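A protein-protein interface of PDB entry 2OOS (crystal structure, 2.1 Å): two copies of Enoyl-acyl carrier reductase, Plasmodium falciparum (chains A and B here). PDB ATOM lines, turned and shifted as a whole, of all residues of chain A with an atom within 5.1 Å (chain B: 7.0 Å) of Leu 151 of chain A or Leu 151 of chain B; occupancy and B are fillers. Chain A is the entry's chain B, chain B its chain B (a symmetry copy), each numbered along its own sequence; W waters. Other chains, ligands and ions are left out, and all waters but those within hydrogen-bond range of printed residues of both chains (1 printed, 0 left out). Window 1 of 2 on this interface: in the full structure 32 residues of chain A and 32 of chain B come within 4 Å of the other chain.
The side-chain hydroxyl of Tyr 147 of chain A sits at hydrogen-bond distance from the side-chain carboxylate of Asp 204 of chain B, 2.6 Å away.
OG of Ser 152 of chain A lies within hydrogen-bond range of NH1 of Arg 144 of chain B (2.8 Å).
The backbone NH (N) of Arg 144 of chain B sits at hydrogen-bond distance from the side-chain hydroxyl (OH) of Tyr 156 of chain A.
The side-chain carboxylate (OD1) of Asp 204 of chain B is in hydrogen-bond range of the side-chain hydroxyl (OG) of Ser 196 of chain A, 2.6 Å away.
The backbone carbonyl oxygen (O) of Leu 151 of chain A is in hydrogen-bond range of the backbone NH (N) of Tyr 156 of chain A (2.9 Å).
N of Ser 157 of chain A lies within hydrogen-bond range of O of Ser 152 of chain A (3.3 Å).
The side-chain hydroxyl (OG) of Ser 155 of chain A lies within hydrogen-bond range of the backbone carbonyl oxygen (O) of Ala 197 of chain A (2.7 Å).
The backbone carbonyl oxygen (O) of Leu 151 of chain B lies within hydrogen-bond range of the backbone NH (N) of Tyr 156 of chain B, 2.9 Å away.
The backbone carbonyl oxygen (O) of Ser 152 of chain B is in hydrogen-bond range of the backbone NH (N) of Ser 157 of chain B (3.3 Å).
OG of Ser 155 of chain B is in hydrogen-bond range of O of Ala 197 of chain B (2.7 Å).
Among the printed residues, pairs that only touch across the chains: Tyr 147 of chain A with Ser 155 of chain B, Ser 155 of chain A with Tyr 147 of chain B, Leu 151 of chain A with Leu 151 of chain B, Leu 148 of chain A with Leu 148 of chain B, Tyr 147 of chain A with Tyr 156 of chain B, Tyr 156 of chain A with Tyr 147 of chain B, Ala 200 of chain A with Tyr 147 of chain B, Tyr 147 of chain A with Ala 200 of chain B, Ser 152 of chain A with Leu 148 of chain B, Leu 148 of chain A with Ser 152 of chain B, Ala 200 of chain A with Ser 196 of chain B and Ser 196 of chain A with Ala 200 of chain B.
Of the printed residues of chain B, Leu 148 of chain A touches Leu 148 and Ser 152.
Ser 157 of chain A touches none of the printed residues of chain B.
Printed residues of chain B within 4 Å of Ser 196 of chain A: Ala 200 (3.98 Å) and Asp 204 (2.6 Å).
Printed residues of chain A within 4 Å of Tyr 147 of chain B: Ser 155, Tyr 156 and Ala 200.
Leu 151 of chain B touches just one residue of chain A: Leu 151 (3.4 Å).
Of the printed residues of chain A, Tyr 156 of chain B touches Tyr 147.
Gly 192 of chain B touches none of the printed residues of chain A.
Printed residues of chain A within 4 Å of Ala 200 of chain B: Tyr 147 (3.6 Å) and Ser 196 (3.98 Å).
Printed residues of chain A that touch a printed residue of chain B: Tyr 147, Leu 148, Leu 151, Ser 152, Ser 155, Tyr 156, Ser 196 and Ala 200.
Hydrophobic or aromatic side chains of chain B that line the printed part of chain A: Tyr 147, Leu 148, Leu 151, Tyr 156 and Ala 200.
Tyr 147 of chain A touches Ser 155 of chain B, and with the chains exchanged Ser 155 of chain A touches Tyr 147 of chain B.
Tyr 147 of chain A touches Ala 200 of chain B, and with the chains exchanged Ala 200 of chain A touches Tyr 147 of chain B.
Leu 148 of chain B touches its own counterpart, Leu 148 of chain A.
Ser 196 of chain A touches Ala 200 of chain B, and with the chains exchanged Ala 200 of chain A touches Ser 196 of chain B.
15 positions are printed for both chains.
Of the 16 pairs that touch across the chains among the printed residues, 12 have their exchanged pair printed and touching as well.
Water W1 lies within hydrogen-bond range of the side-chain carboxylate (OD1) of Asp 204 of chain B (2.7 Å) and the backbone NH (N) of Ser 196 of chain A (3.4 Å).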
ATOM      1  N   TYR A 147      -1.193  26.452   4.873  1.00  0.00           N
ATOM      2  CA  TYR A 147      -1.976  26.374   3.608  1.00  0.00           C
ATOM      3  C   TYR A 147      -2.559  27.745   3.304  1.00  0.00           C
ATOM      4  O   TYR A 147      -2.447  28.235   2.204  1.00  0.00           O
ATOM      5  CB  TYR A 147      -3.138  25.430   3.825  1.00  0.00           C
ATOM      6  CG  TYR A 147      -4.045  25.130   2.646  1.00  0.00           C
ATOM      7  CD1 TYR A 147      -5.266  25.806   2.478  1.00  0.00           C
ATOM      8  CD2 TYR A 147      -3.701  24.142   1.709  1.00  0.00           C
ATOM      9  CE1 TYR A 147      -6.141  25.470   1.399  1.00  0.00           C
ATOM     10  CE2 TYR A 147      -4.553  23.816   0.670  1.00  0.00           C
ATOM     11  CZ  TYR A 147      -5.776  24.489   0.512  1.00  0.00           C
ATOM     12  OH  TYR A 147      -6.633  24.155  -0.535  1.00  0.00           O
ATOM     13  N   LEU A 148      -3.193  28.345   4.302  1.00  0.00           N
ATOM     14  CA  LEU A 148      -3.770  29.674   4.115  1.00  0.00           C
ATOM     15  C   LEU A 148      -2.721  30.743   3.856  1.00  0.00           C
ATOM     16  O   LEU A 148      -2.999  31.711   3.169  1.00  0.00           O
ATOM     17  CB  LEU A 148      -4.657  30.081   5.301  1.00  0.00           C
ATOM     18  CG  LEU A 148      -5.889  29.211   5.523  1.00  0.00           C
ATOM     19  CD1 LEU A 148      -6.602  29.707   6.792  1.00  0.00           C
ATOM     20  CD2 LEU A 148      -6.817  29.246   4.317  1.00  0.00           C
ATOM     21  N   ASP A 149      -1.512  30.561   4.391  1.00  0.00           N
ATOM     22  CA  ASP A 149      -0.406  31.476   4.082  1.00  0.00           C
ATOM     23  C   ASP A 149      -0.003  31.365   2.605  1.00  0.00           C
ATOM     24  O   ASP A 149       0.195  32.380   1.958  1.00  0.00           O
ATOM     25  CB  ASP A 149       0.816  31.175   4.953  1.00  0.00           C
ATOM     26  CG  ASP A 149       1.972  32.080   4.651  1.00  0.00           C
ATOM     27  OD1 ASP A 149       2.903  31.633   3.923  1.00  0.00           O
ATOM     28  OD2 ASP A 149       1.939  33.253   5.106  1.00  0.00           O
ATOM     29  N   ALA A 150       0.079  30.145   2.071  1.00  0.00           N
ATOM     30  CA  ALA A 150       0.332  29.945   0.632  1.00  0.00           C
ATOM     31  C   ALA A 150      -0.757  30.603  -0.224  1.00  0.00           C
ATOM     32  O   ALA A 150      -0.462  31.267  -1.183  1.00  0.00           O
ATOM     33  CB  ALA A 150       0.465  28.422   0.293  1.00  0.00           C
ATOM     34  N   LEU A 151      -2.023  30.416   0.139  1.00  0.00           N
ATOM     35  CA  LEU A 151      -3.127  31.040  -0.627  1.00  0.00           C
ATOM     36  C   LEU A 151      -3.117  32.571  -0.518  1.00  0.00           C
ATOM     37  O   LEU A 151      -3.261  33.273  -1.509  1.00  0.00           O
ATOM     38  CB  LEU A 151      -4.476  30.376  -0.233  1.00  0.00           C
ATOM     39  CG  LEU A 151      -4.452  29.237  -1.275  1.00  0.00           C
ATOM     40  CD1 LEU A 151      -4.096  27.815  -0.835  1.00  0.00           C
ATOM     41  CD2 LEU A 151      -5.501  29.341  -2.422  1.00  0.00           C
ATOM     42  N   SER A 152      -2.908  33.078   0.698  1.00  0.00           N
ATOM     43  CA  SER A 152      -2.759  34.503   0.883  1.00  0.00           C
ATOM     44  C   SER A 152      -1.679  35.177   0.071  1.00  0.00           C
ATOM     45  O   SER A 152      -1.933  36.161  -0.644  1.00  0.00           O
ATOM     46  CB  SER A 152      -2.591  34.839   2.369  1.00  0.00           C
ATOM     47  OG  SER A 152      -2.578  36.212   2.494  1.00  0.00           O
ATOM     48  N   LYS A 153      -0.456  34.654   0.159  1.00  0.00           N
ATOM     49  CA  LYS A 153       0.671  35.285  -0.540  1.00  0.00           C
ATOM     50  C   LYS A 153       0.727  35.021  -2.065  1.00  0.00           C
ATOM     51  O   LYS A 153       1.139  35.877  -2.853  1.00  0.00           O
ATOM     52  CB  LYS A 153       2.006  34.869   0.109  1.00  0.00           C
ATOM     53  CG  LYS A 153       2.118  35.061   1.658  1.00  0.00           C
ATOM     54  CD  LYS A 153       1.639  36.412   2.192  1.00  0.00           C
ATOM     55  CE  LYS A 153       1.856  36.505   3.757  1.00  0.00           C
ATOM     56  NZ  LYS A 153       3.154  35.799   4.160  1.00  0.00           N
ATOM     57  N   SER A 154       0.344  33.829  -2.484  1.00  0.00           N
ATOM     58  CA  SER A 154       0.530  33.445  -3.883  1.00  0.00           C
ATOM     59  C   SER A 154      -0.696  33.613  -4.794  1.00  0.00           C
ATOM     60  O   SER A 154      -0.529  33.649  -6.022  1.00  0.00           O
ATOM     61  CB  SER A 154       0.980  31.981  -3.961  1.00  0.00           C
ATOM     62  OG  SER A 154       2.107  31.791  -3.106  1.00  0.00           O
ATOM     63  N   SER A 155      -1.895  33.654  -4.204  1.00  0.00           N
ATOM     64  CA  SER A 155      -3.154  33.693  -4.978  1.00  0.00           C
ATOM     65  C   SER A 155      -3.941  34.978  -4.680  1.00  0.00           C
ATOM     66  O   SER A 155      -4.270  35.739  -5.589  1.00  0.00           O
ATOM     67  CB  SER A 155      -4.061  32.481  -4.657  1.00  0.00           C
ATOM     68  OG  SER A 155      -3.323  31.282  -4.737  1.00  0.00           O
ATOM     69  N   TYR A 156      -4.288  35.183  -3.415  1.00  0.00           N
ATOM     70  CA  TYR A 156      -5.061  36.368  -3.079  1.00  0.00           C
ATOM     71  C   TYR A 156      -4.328  37.661  -3.484  1.00  0.00           C
ATOM     72  O   TYR A 156      -4.955  38.601  -3.901  1.00  0.00           O
ATOM     73  CB  TYR A 156      -5.508  36.429  -1.585  1.00  0.00           C
ATOM     74  CG  TYR A 156      -6.376  37.627  -1.427  1.00  0.00           C
ATOM     75  CD1 TYR A 156      -7.694  37.615  -1.904  1.00  0.00           C
ATOM     76  CD2 TYR A 156      -5.866  38.827  -0.911  1.00  0.00           C
ATOM     77  CE1 TYR A 156      -8.505  38.762  -1.839  1.00  0.00           C
ATOM     78  CE2 TYR A 156      -6.683  39.985  -0.812  1.00  0.00           C
ATOM     79  CZ  TYR A 156      -7.973  39.948  -1.302  1.00  0.00           C
ATOM     80  OH  TYR A 156      -8.768  41.078  -1.227  1.00  0.00           O
ATOM     81  N   SER A 157      -3.006  37.694  -3.355  1.00  0.00           N
ATOM     82  CA  SER A 157      -2.176  38.852  -3.719  1.00  0.00           C
ATOM     83  C   SER A 157      -2.434  39.309  -5.168  1.00  0.00           C
ATOM     84  O   SER A 157      -2.362  40.523  -5.448  1.00  0.00           O
ATOM     85  CB  SER A 157      -0.686  38.527  -3.557  1.00  0.00           C
ATOM     86  OG  SER A 157      -0.329  37.351  -4.297  1.00  0.00           O
ATOM     87  N   GLY A 193       0.660  23.582   0.221  1.00  0.00           N
ATOM     88  CA  GLY A 193      -0.444  24.325  -0.425  1.00  0.00           C
ATOM     89  C   GLY A 193      -0.041  25.146  -1.670  1.00  0.00           C
ATOM     90  O   GLY A 193      -0.864  25.903  -2.197  1.00  0.00           O
ATOM     91  N   SER A 196      -2.066  23.938  -4.535  1.00  0.00           N
ATOM     92  CA  SER A 196      -3.416  24.512  -4.275  1.00  0.00           C
ATOM     93  C   SER A 196      -3.494  26.004  -4.656  1.00  0.00           C
ATOM     94  O   SER A 196      -4.465  26.458  -5.269  1.00  0.00           O
ATOM     95  CB  SER A 196      -3.744  24.365  -2.791  1.00  0.00           C
ATOM     96  OG  SER A 196      -3.179  23.142  -2.316  1.00  0.00           O
ATOM     97  N   ALA A 197      -2.477  26.760  -4.264  1.00  0.00           N
ATOM     98  CA  ALA A 197      -2.408  28.173  -4.587  1.00  0.00           C
ATOM     99  C   ALA A 197      -2.354  28.413  -6.103  1.00  0.00           C
ATOM    100  O   ALA A 197      -2.921  29.370  -6.579  1.00  0.00           O
ATOM    101  CB  ALA A 197      -1.175  28.803  -3.913  1.00  0.00           C
ATOM    102  N   ALA A 200      -5.765  27.668  -7.581  1.00  0.00           N
ATOM    103  CA  ALA A 200      -6.628  28.839  -7.317  1.00  0.00           C
ATOM    104  C   ALA A 200      -6.292  30.026  -8.215  1.00  0.00           C
ATOM    105  O   ALA A 200      -7.178  30.613  -8.755  1.00  0.00           O
ATOM    106  CB  ALA A 200      -6.565  29.249  -5.829  1.00  0.00           C
ATOM    107  N   ASN B 131     -18.349  26.796   2.891  1.00  0.00           N
ATOM    108  CA  ASN B 131     -18.715  27.999   3.608  1.00  0.00           C
ATOM    109  C   ASN B 131     -17.809  29.088   3.145  1.00  0.00           C
ATOM    110  O   ASN B 131     -16.641  28.832   2.769  1.00  0.00           O
ATOM    111  CB  ASN B 131     -18.561  27.786   5.111  1.00  0.00           C
ATOM    112  CG  ASN B 131     -19.747  28.331   5.907  1.00  0.00           C
ATOM    113  OD1 ASN B 131     -20.899  27.922   5.743  1.00  0.00           O
ATOM    114  ND2 ASN B 131     -19.451  29.256   6.781  1.00  0.00           N
ATOM    115  N   ALA B 132     -18.345  30.312   3.121  1.00  0.00           N
ATOM    116  CA  ALA B 132     -17.576  31.485   2.648  1.00  0.00           C
ATOM    117  C   ALA B 132     -18.299  32.755   3.110  1.00  0.00           C
ATOM    118  O   ALA B 132     -19.394  33.028   2.673  1.00  0.00           O
ATOM    119  CB  ALA B 132     -17.440  31.467   1.114  1.00  0.00           C
ATOM    120  N   ARG B 144      -9.280  39.821   1.712  1.00  0.00           N
ATOM    121  CA  ARG B 144      -8.316  38.766   2.011  1.00  0.00           C
ATOM    122  C   ARG B 144      -8.919  37.825   3.049  1.00  0.00           C
ATOM    123  O   ARG B 144      -8.918  36.600   2.889  1.00  0.00           O
ATOM    124  CB  ARG B 144      -6.975  39.360   2.460  1.00  0.00           C
ATOM    125  CG  ARG B 144      -5.826  38.338   2.576  1.00  0.00           C
ATOM    126  CD  ARG B 144      -4.495  39.030   2.964  1.00  0.00           C
ATOM    127  NE  ARG B 144      -4.058  39.983   1.928  1.00  0.00           N
ATOM    128  CZ  ARG B 144      -3.090  39.781   1.047  1.00  0.00           C
ATOM    129  NH1 ARG B 144      -2.391  38.628   1.014  1.00  0.00           N
ATOM    130  NH2 ARG B 144      -2.811  40.755   0.188  1.00  0.00           N
ATOM    131  N   GLY B 146     -12.132  37.331   3.719  1.00  0.00           N
ATOM    132  CA  GLY B 146     -13.235  36.543   3.140  1.00  0.00           C
ATOM    133  C   GLY B 146     -12.708  35.372   2.273  1.00  0.00           C
ATOM    134  O   GLY B 146     -13.201  34.238   2.367  1.00  0.00           O
ATOM    135  N   TYR B 147     -11.731  35.658   1.418  1.00  0.00           N
ATOM    136  CA  TYR B 147     -11.162  34.661   0.469  1.00  0.00           C
ATOM    137  C   TYR B 147     -10.531  33.529   1.265  1.00  0.00           C
ATOM    138  O   TYR B 147     -10.775  32.374   0.999  1.00  0.00           O
ATOM    139  CB  TYR B 147     -10.054  35.328  -0.317  1.00  0.00           C
ATOM    140  CG  TYR B 147      -9.367  34.525  -1.406  1.00  0.00           C
ATOM    141  CD1 TYR B 147      -8.140  33.883  -1.171  1.00  0.00           C
ATOM    142  CD2 TYR B 147      -9.926  34.434  -2.691  1.00  0.00           C
ATOM    143  CE1 TYR B 147      -7.471  33.183  -2.222  1.00  0.00           C
ATOM    144  CE2 TYR B 147      -9.274  33.760  -3.707  1.00  0.00           C
ATOM    145  CZ  TYR B 147      -8.043  33.126  -3.468  1.00  0.00           C
ATOM    146  OH  TYR B 147      -7.388  32.451  -4.496  1.00  0.00           O
ATOM    147  N   LEU B 148      -9.706  33.887   2.239  1.00  0.00           N
ATOM    148  CA  LEU B 148      -9.066  32.873   3.073  1.00  0.00           C
ATOM    149  C   LEU B 148     -10.059  32.087   3.914  1.00  0.00           C
ATOM    150  O   LEU B 148      -9.818  30.929   4.209  1.00  0.00           O
ATOM    151  CB  LEU B 148      -7.978  33.479   3.971  1.00  0.00           C
ATOM    152  CG  LEU B 148      -6.795  34.098   3.235  1.00  0.00           C
ATOM    153  CD1 LEU B 148      -5.858  34.728   4.279  1.00  0.00           C
ATOM    154  CD2 LEU B 148      -6.066  33.065   2.388  1.00  0.00           C
ATOM    155  N   ASP B 149     -11.181  32.708   4.284  1.00  0.00           N
ATOM    156  CA  ASP B 149     -12.248  31.984   4.982  1.00  0.00           C
ATOM    157  C   ASP B 149     -12.884  30.929   4.064  1.00  0.00           C
ATOM    158  O   ASP B 149     -13.102  29.810   4.495  1.00  0.00           O
ATOM    159  CB  ASP B 149     -13.340  32.942   5.465  1.00  0.00           C
ATOM    160  CG  ASP B 149     -14.457  32.232   6.169  1.00  0.00           C
ATOM    161  OD1 ASP B 149     -15.521  32.011   5.524  1.00  0.00           O
ATOM    162  OD2 ASP B 149     -14.265  31.857   7.355  1.00  0.00           O
ATOM    163  N   ALA B 150     -13.140  31.276   2.802  1.00  0.00           N
ATOM    164  CA  ALA B 150     -13.628  30.296   1.813  1.00  0.00           C
ATOM    165  C   ALA B 150     -12.639  29.137   1.639  1.00  0.00           C
ATOM    166  O   ALA B 150     -13.029  27.999   1.623  1.00  0.00           O
ATOM    167  CB  ALA B 150     -13.926  30.987   0.441  1.00  0.00           C
ATOM    168  N   LEU B 151     -11.349  29.441   1.516  1.00  0.00           N
ATOM    169  CA  LEU B 151     -10.334  28.373   1.368  1.00  0.00           C
ATOM    170  C   LEU B 151     -10.211  27.508   2.630  1.00  0.00           C
ATOM    171  O   LEU B 151     -10.171  26.288   2.556  1.00  0.00           O
ATOM    172  CB  LEU B 151      -8.995  28.990   0.879  1.00  0.00           C
ATOM    173  CG  LEU B 151      -9.266  28.886  -0.638  1.00  0.00           C
ATOM    174  CD1 LEU B 151      -9.656  30.139  -1.426  1.00  0.00           C
ATOM    175  CD2 LEU B 151      -8.404  27.846  -1.414  1.00  0.00           C
ATOM    176  N   SER B 152     -10.190  28.158   3.794  1.00  0.00           N
ATOM    177  CA  SER B 152     -10.199  27.430   5.043  1.00  0.00           C
ATOM    178  C   SER B 152     -11.339  26.459   5.245  1.00  0.00           C
ATOM    179  O   SER B 152     -11.125  25.272   5.540  1.00  0.00           O
ATOM    180  CB  SER B 152     -10.108  28.394   6.231  1.00  0.00           C
ATOM    181  OG  SER B 152      -9.998  27.641   7.380  1.00  0.00           O
ATOM    182  N   LYS B 153     -12.569  26.945   5.080  1.00  0.00           N
ATOM    183  CA  LYS B 153     -13.740  26.093   5.325  1.00  0.00           C
ATOM    184  C   LYS B 153     -14.053  25.071   4.204  1.00  0.00           C
ATOM    185  O   LYS B 153     -14.516  23.956   4.459  1.00  0.00           O
ATOM    186  CB  LYS B 153     -14.986  26.959   5.601  1.00  0.00           C
ATOM    187  CG  LYS B 153     -14.841  28.057   6.705  1.00  0.00           C
ATOM    188  CD  LYS B 153     -14.184  27.599   8.009  1.00  0.00           C
ATOM    189  CE  LYS B 153     -14.147  28.780   9.063  1.00  0.00           C
ATOM    190  NZ  LYS B 153     -15.416  29.632   8.958  1.00  0.00           N
ATOM    191  N   SER B 154     -13.831  25.455   2.960  1.00  0.00           N
ATOM    192  CA  SER B 154     -14.260  24.615   1.843  1.00  0.00           C
ATOM    193  C   SER B 154     -13.182  23.707   1.231  1.00  0.00           C
ATOM    194  O   SER B 154     -13.534  22.740   0.542  1.00  0.00           O
ATOM    195  CB  SER B 154     -14.826  25.497   0.723  1.00  0.00           C
ATOM    196  OG  SER B 154     -15.818  26.368   1.266  1.00  0.00           O
ATOM    197  N   SER B 155     -11.906  24.052   1.434  1.00  0.00           N
ATOM    198  CA  SER B 155     -10.783  23.328   0.800  1.00  0.00           C
ATOM    199  C   SER B 155      -9.865  22.704   1.861  1.00  0.00           C
ATOM    200  O   SER B 155      -9.624  21.498   1.853  1.00  0.00           O
ATOM    201  CB  SER B 155      -9.932  24.262  -0.093  1.00  0.00           C
ATOM    202  OG  SER B 155     -10.762  25.000  -0.962  1.00  0.00           O
ATOM    203  N   TYR B 156      -9.311  23.537   2.733  1.00  0.00           N
ATOM    204  CA  TYR B 156      -8.407  23.006   3.741  1.00  0.00           C
ATOM    205  C   TYR B 156      -9.095  21.943   4.619  1.00  0.00           C
ATOM    206  O   TYR B 156      -8.472  20.987   5.003  1.00  0.00           O
ATOM    207  CB  TYR B 156      -7.730  24.101   4.624  1.00  0.00           C
ATOM    208  CG  TYR B 156      -6.760  23.415   5.520  1.00  0.00           C
ATOM    209  CD1 TYR B 156      -5.537  22.951   5.016  1.00  0.00           C
ATOM    210  CD2 TYR B 156      -7.092  23.111   6.848  1.00  0.00           C
ATOM    211  CE1 TYR B 156      -4.642  22.227   5.825  1.00  0.00           C
ATOM    212  CE2 TYR B 156      -6.184  22.410   7.684  1.00  0.00           C
ATOM    213  CZ  TYR B 156      -4.993  21.951   7.158  1.00  0.00           C
ATOM    214  OH  TYR B 156      -4.113  21.248   7.962  1.00  0.00           O
ATOM    215  N   SER B 157     -10.374  22.123   4.929  1.00  0.00           N
ATOM    216  CA  SER B 157     -11.161  21.183   5.741  1.00  0.00           C
ATOM    217  C   SER B 157     -11.097  19.750   5.179  1.00  0.00           C
ATOM    218  O   SER B 157     -11.120  18.784   5.969  1.00  0.00           O
ATOM    219  CB  SER B 157     -12.627  21.624   5.817  1.00  0.00           C
ATOM    220  OG  SER B 157     -13.183  21.803   4.507  1.00  0.00           O
ATOM    221  N   LEU B 158     -10.978  19.633   3.845  1.00  0.00           N
ATOM    222  CA  LEU B 158     -10.835  18.319   3.211  1.00  0.00           C
ATOM    223  C   LEU B 158      -9.490  17.699   3.538  1.00  0.00           C
ATOM    224  O   LEU B 158      -9.424  16.531   3.871  1.00  0.00           O
ATOM    225  CB  LEU B 158     -11.040  18.369   1.678  1.00  0.00           C
ATOM    226  CG  LEU B 158     -10.729  17.048   0.952  1.00  0.00           C
ATOM    227  CD1 LEU B 158     -11.733  15.990   1.369  1.00  0.00           C
ATOM    228  CD2 LEU B 158     -10.674  17.188  -0.556  1.00  0.00           C
ATOM    229  N   GLY B 192     -17.042  35.312  -3.575  1.00  0.00           N
ATOM    230  CA  GLY B 192     -16.328  35.190  -2.283  1.00  0.00           C
ATOM    231  C   GLY B 192     -15.098  34.284  -2.211  1.00  0.00           C
ATOM    232  O   GLY B 192     -14.679  33.903  -1.119  1.00  0.00           O
ATOM    233  N   GLY B 193     -14.496  33.949  -3.351  1.00  0.00           N
ATOM    234  CA  GLY B 193     -13.453  32.900  -3.334  1.00  0.00           C
ATOM    235  C   GLY B 193     -13.981  31.449  -3.384  1.00  0.00           C
ATOM    236  O   GLY B 193     -13.195  30.506  -3.240  1.00  0.00           O
ATOM    237  N   MET B 194     -15.297  31.258  -3.540  1.00  0.00           N
ATOM    238  CA  MET B 194     -15.846  29.915  -3.667  1.00  0.00           C
ATOM    239  C   MET B 194     -15.361  29.200  -4.928  1.00  0.00           C
ATOM    240  O   MET B 194     -15.150  27.975  -4.913  1.00  0.00           O
ATOM    241  CB  MET B 194     -17.363  29.869  -3.588  1.00  0.00           C
ATOM    242  CG  MET B 194     -17.955  29.754  -2.135  1.00  0.00           C
ATOM    243  SD  MET B 194     -17.232  28.462  -1.068  1.00  0.00           S
ATOM    244  CE  MET B 194     -17.524  26.957  -1.996  1.00  0.00           C
ATOM    245  N   SER B 195     -15.243  29.955  -6.013  1.00  0.00           N
ATOM    246  CA  SER B 195     -14.746  29.390  -7.255  1.00  0.00           C
ATOM    247  C   SER B 195     -13.290  28.930  -7.017  1.00  0.00           C
ATOM    248  O   SER B 195     -12.890  27.824  -7.445  1.00  0.00           O
ATOM    249  CB  SER B 195     -14.810  30.438  -8.378  1.00  0.00           C
ATOM    250  OG  SER B 195     -14.010  31.600  -8.050  1.00  0.00           O
ATOM    251  N   SER B 196     -12.524  29.810  -6.376  1.00  0.00           N
ATOM    252  CA  SER B 196     -11.110  29.554  -5.981  1.00  0.00           C
ATOM    253  C   SER B 196     -10.980  28.326  -5.060  1.00  0.00           C
ATOM    254  O   SER B 196     -10.084  27.492  -5.227  1.00  0.00           O
ATOM    255  CB  SER B 196     -10.568  30.780  -5.248  1.00  0.00           C
ATOM    256  OG  SER B 196     -11.143  31.952  -5.827  1.00  0.00           O
ATOM    257  N   ALA B 197     -11.864  28.239  -4.074  1.00  0.00           N
ATOM    258  CA  ALA B 197     -11.875  27.116  -3.156  1.00  0.00           C
ATOM    259  C   ALA B 197     -12.146  25.788  -3.878  1.00  0.00           C
ATOM    260  O   ALA B 197     -11.589  24.780  -3.508  1.00  0.00           O
ATOM    261  CB  ALA B 197     -12.936  27.344  -2.064  1.00  0.00           C
ATOM    262  N   LYS B 198     -13.080  25.770  -4.841  1.00  0.00           N
ATOM    263  CA  LYS B 198     -13.349  24.539  -5.569  1.00  0.00           C
ATOM    264  C   LYS B 198     -12.204  24.154  -6.544  1.00  0.00           C
ATOM    265  O   LYS B 198     -11.946  22.977  -6.770  1.00  0.00           O
ATOM    266  CB  LYS B 198     -14.682  24.641  -6.339  1.00  0.00           C
ATOM    267  CG  LYS B 198     -15.925  24.784  -5.425  1.00  0.00           C
ATOM    268  CD  LYS B 198     -16.032  23.636  -4.397  1.00  0.00           C
ATOM    269  CE  LYS B 198     -17.462  23.554  -3.840  1.00  0.00           C
ATOM    270  NZ  LYS B 198     -17.554  22.642  -2.663  1.00  0.00           N
ATOM    271  N   ALA B 199     -11.560  25.156  -7.159  1.00  0.00           N
ATOM    272  CA  ALA B 199     -10.393  24.868  -7.968  1.00  0.00           C
ATOM    273  C   ALA B 199      -9.313  24.240  -7.056  1.00  0.00           C
ATOM    274  O   ALA B 199      -8.676  23.274  -7.449  1.00  0.00           O
ATOM    275  CB  ALA B 199      -9.862  26.154  -8.631  1.00  0.00           C
ATOM    276  N   ALA B 200      -9.072  24.838  -5.885  1.00  0.00           N
ATOM    277  CA  ALA B 200      -8.093  24.252  -4.945  1.00  0.00           C
ATOM    278  C   ALA B 200      -8.473  22.840  -4.510  1.00  0.00           C
ATOM    279  O   ALA B 200      -7.640  21.987  -4.516  1.00  0.00           O
ATOM    280  CB  ALA B 200      -7.892  25.164  -3.714  1.00  0.00           C
ATOM    281  N   LEU B 201      -9.749  22.599  -4.177  1.00  0.00           N
ATOM    282  CA  LEU B 201     -10.216  21.289  -3.794  1.00  0.00           C
ATOM    283  C   LEU B 201     -10.000  20.249  -4.913  1.00  0.00           C
ATOM    284  O   LEU B 201      -9.662  19.128  -4.606  1.00  0.00           O
ATOM    285  CB  LEU B 201     -11.713  21.337  -3.395  1.00  0.00           C
ATOM    286  CG  LEU B 201     -12.564  20.121  -2.978  1.00  0.00           C
ATOM    287  CD1 LEU B 201     -12.362  19.948  -1.538  1.00  0.00           C
ATOM    288  CD2 LEU B 201     -14.108  20.289  -3.108  1.00  0.00           C
ATOM    289  N   ASP B 204      -6.192  19.607  -5.052  1.00  0.00           N
ATOM    290  CA  ASP B 204      -5.838  18.871  -3.799  1.00  0.00           C
ATOM    291  C   ASP B 204      -6.310  17.433  -3.824  1.00  0.00           C
ATOM    292  O   ASP B 204      -5.688  16.568  -3.226  1.00  0.00           O
ATOM    293  CB  ASP B 204      -6.408  19.545  -2.534  1.00  0.00           C
ATOM    294  CG  ASP B 204      -5.854  20.966  -2.317  1.00  0.00           C
ATOM    295  OD1 ASP B 204      -4.847  21.323  -3.011  1.00  0.00           O
ATOM    296  OD2 ASP B 204      -6.446  21.712  -1.477  1.00  0.00           O
HETATM  297  O   HOH W   1      -3.145  20.720  -4.974  1.00  0.00           O
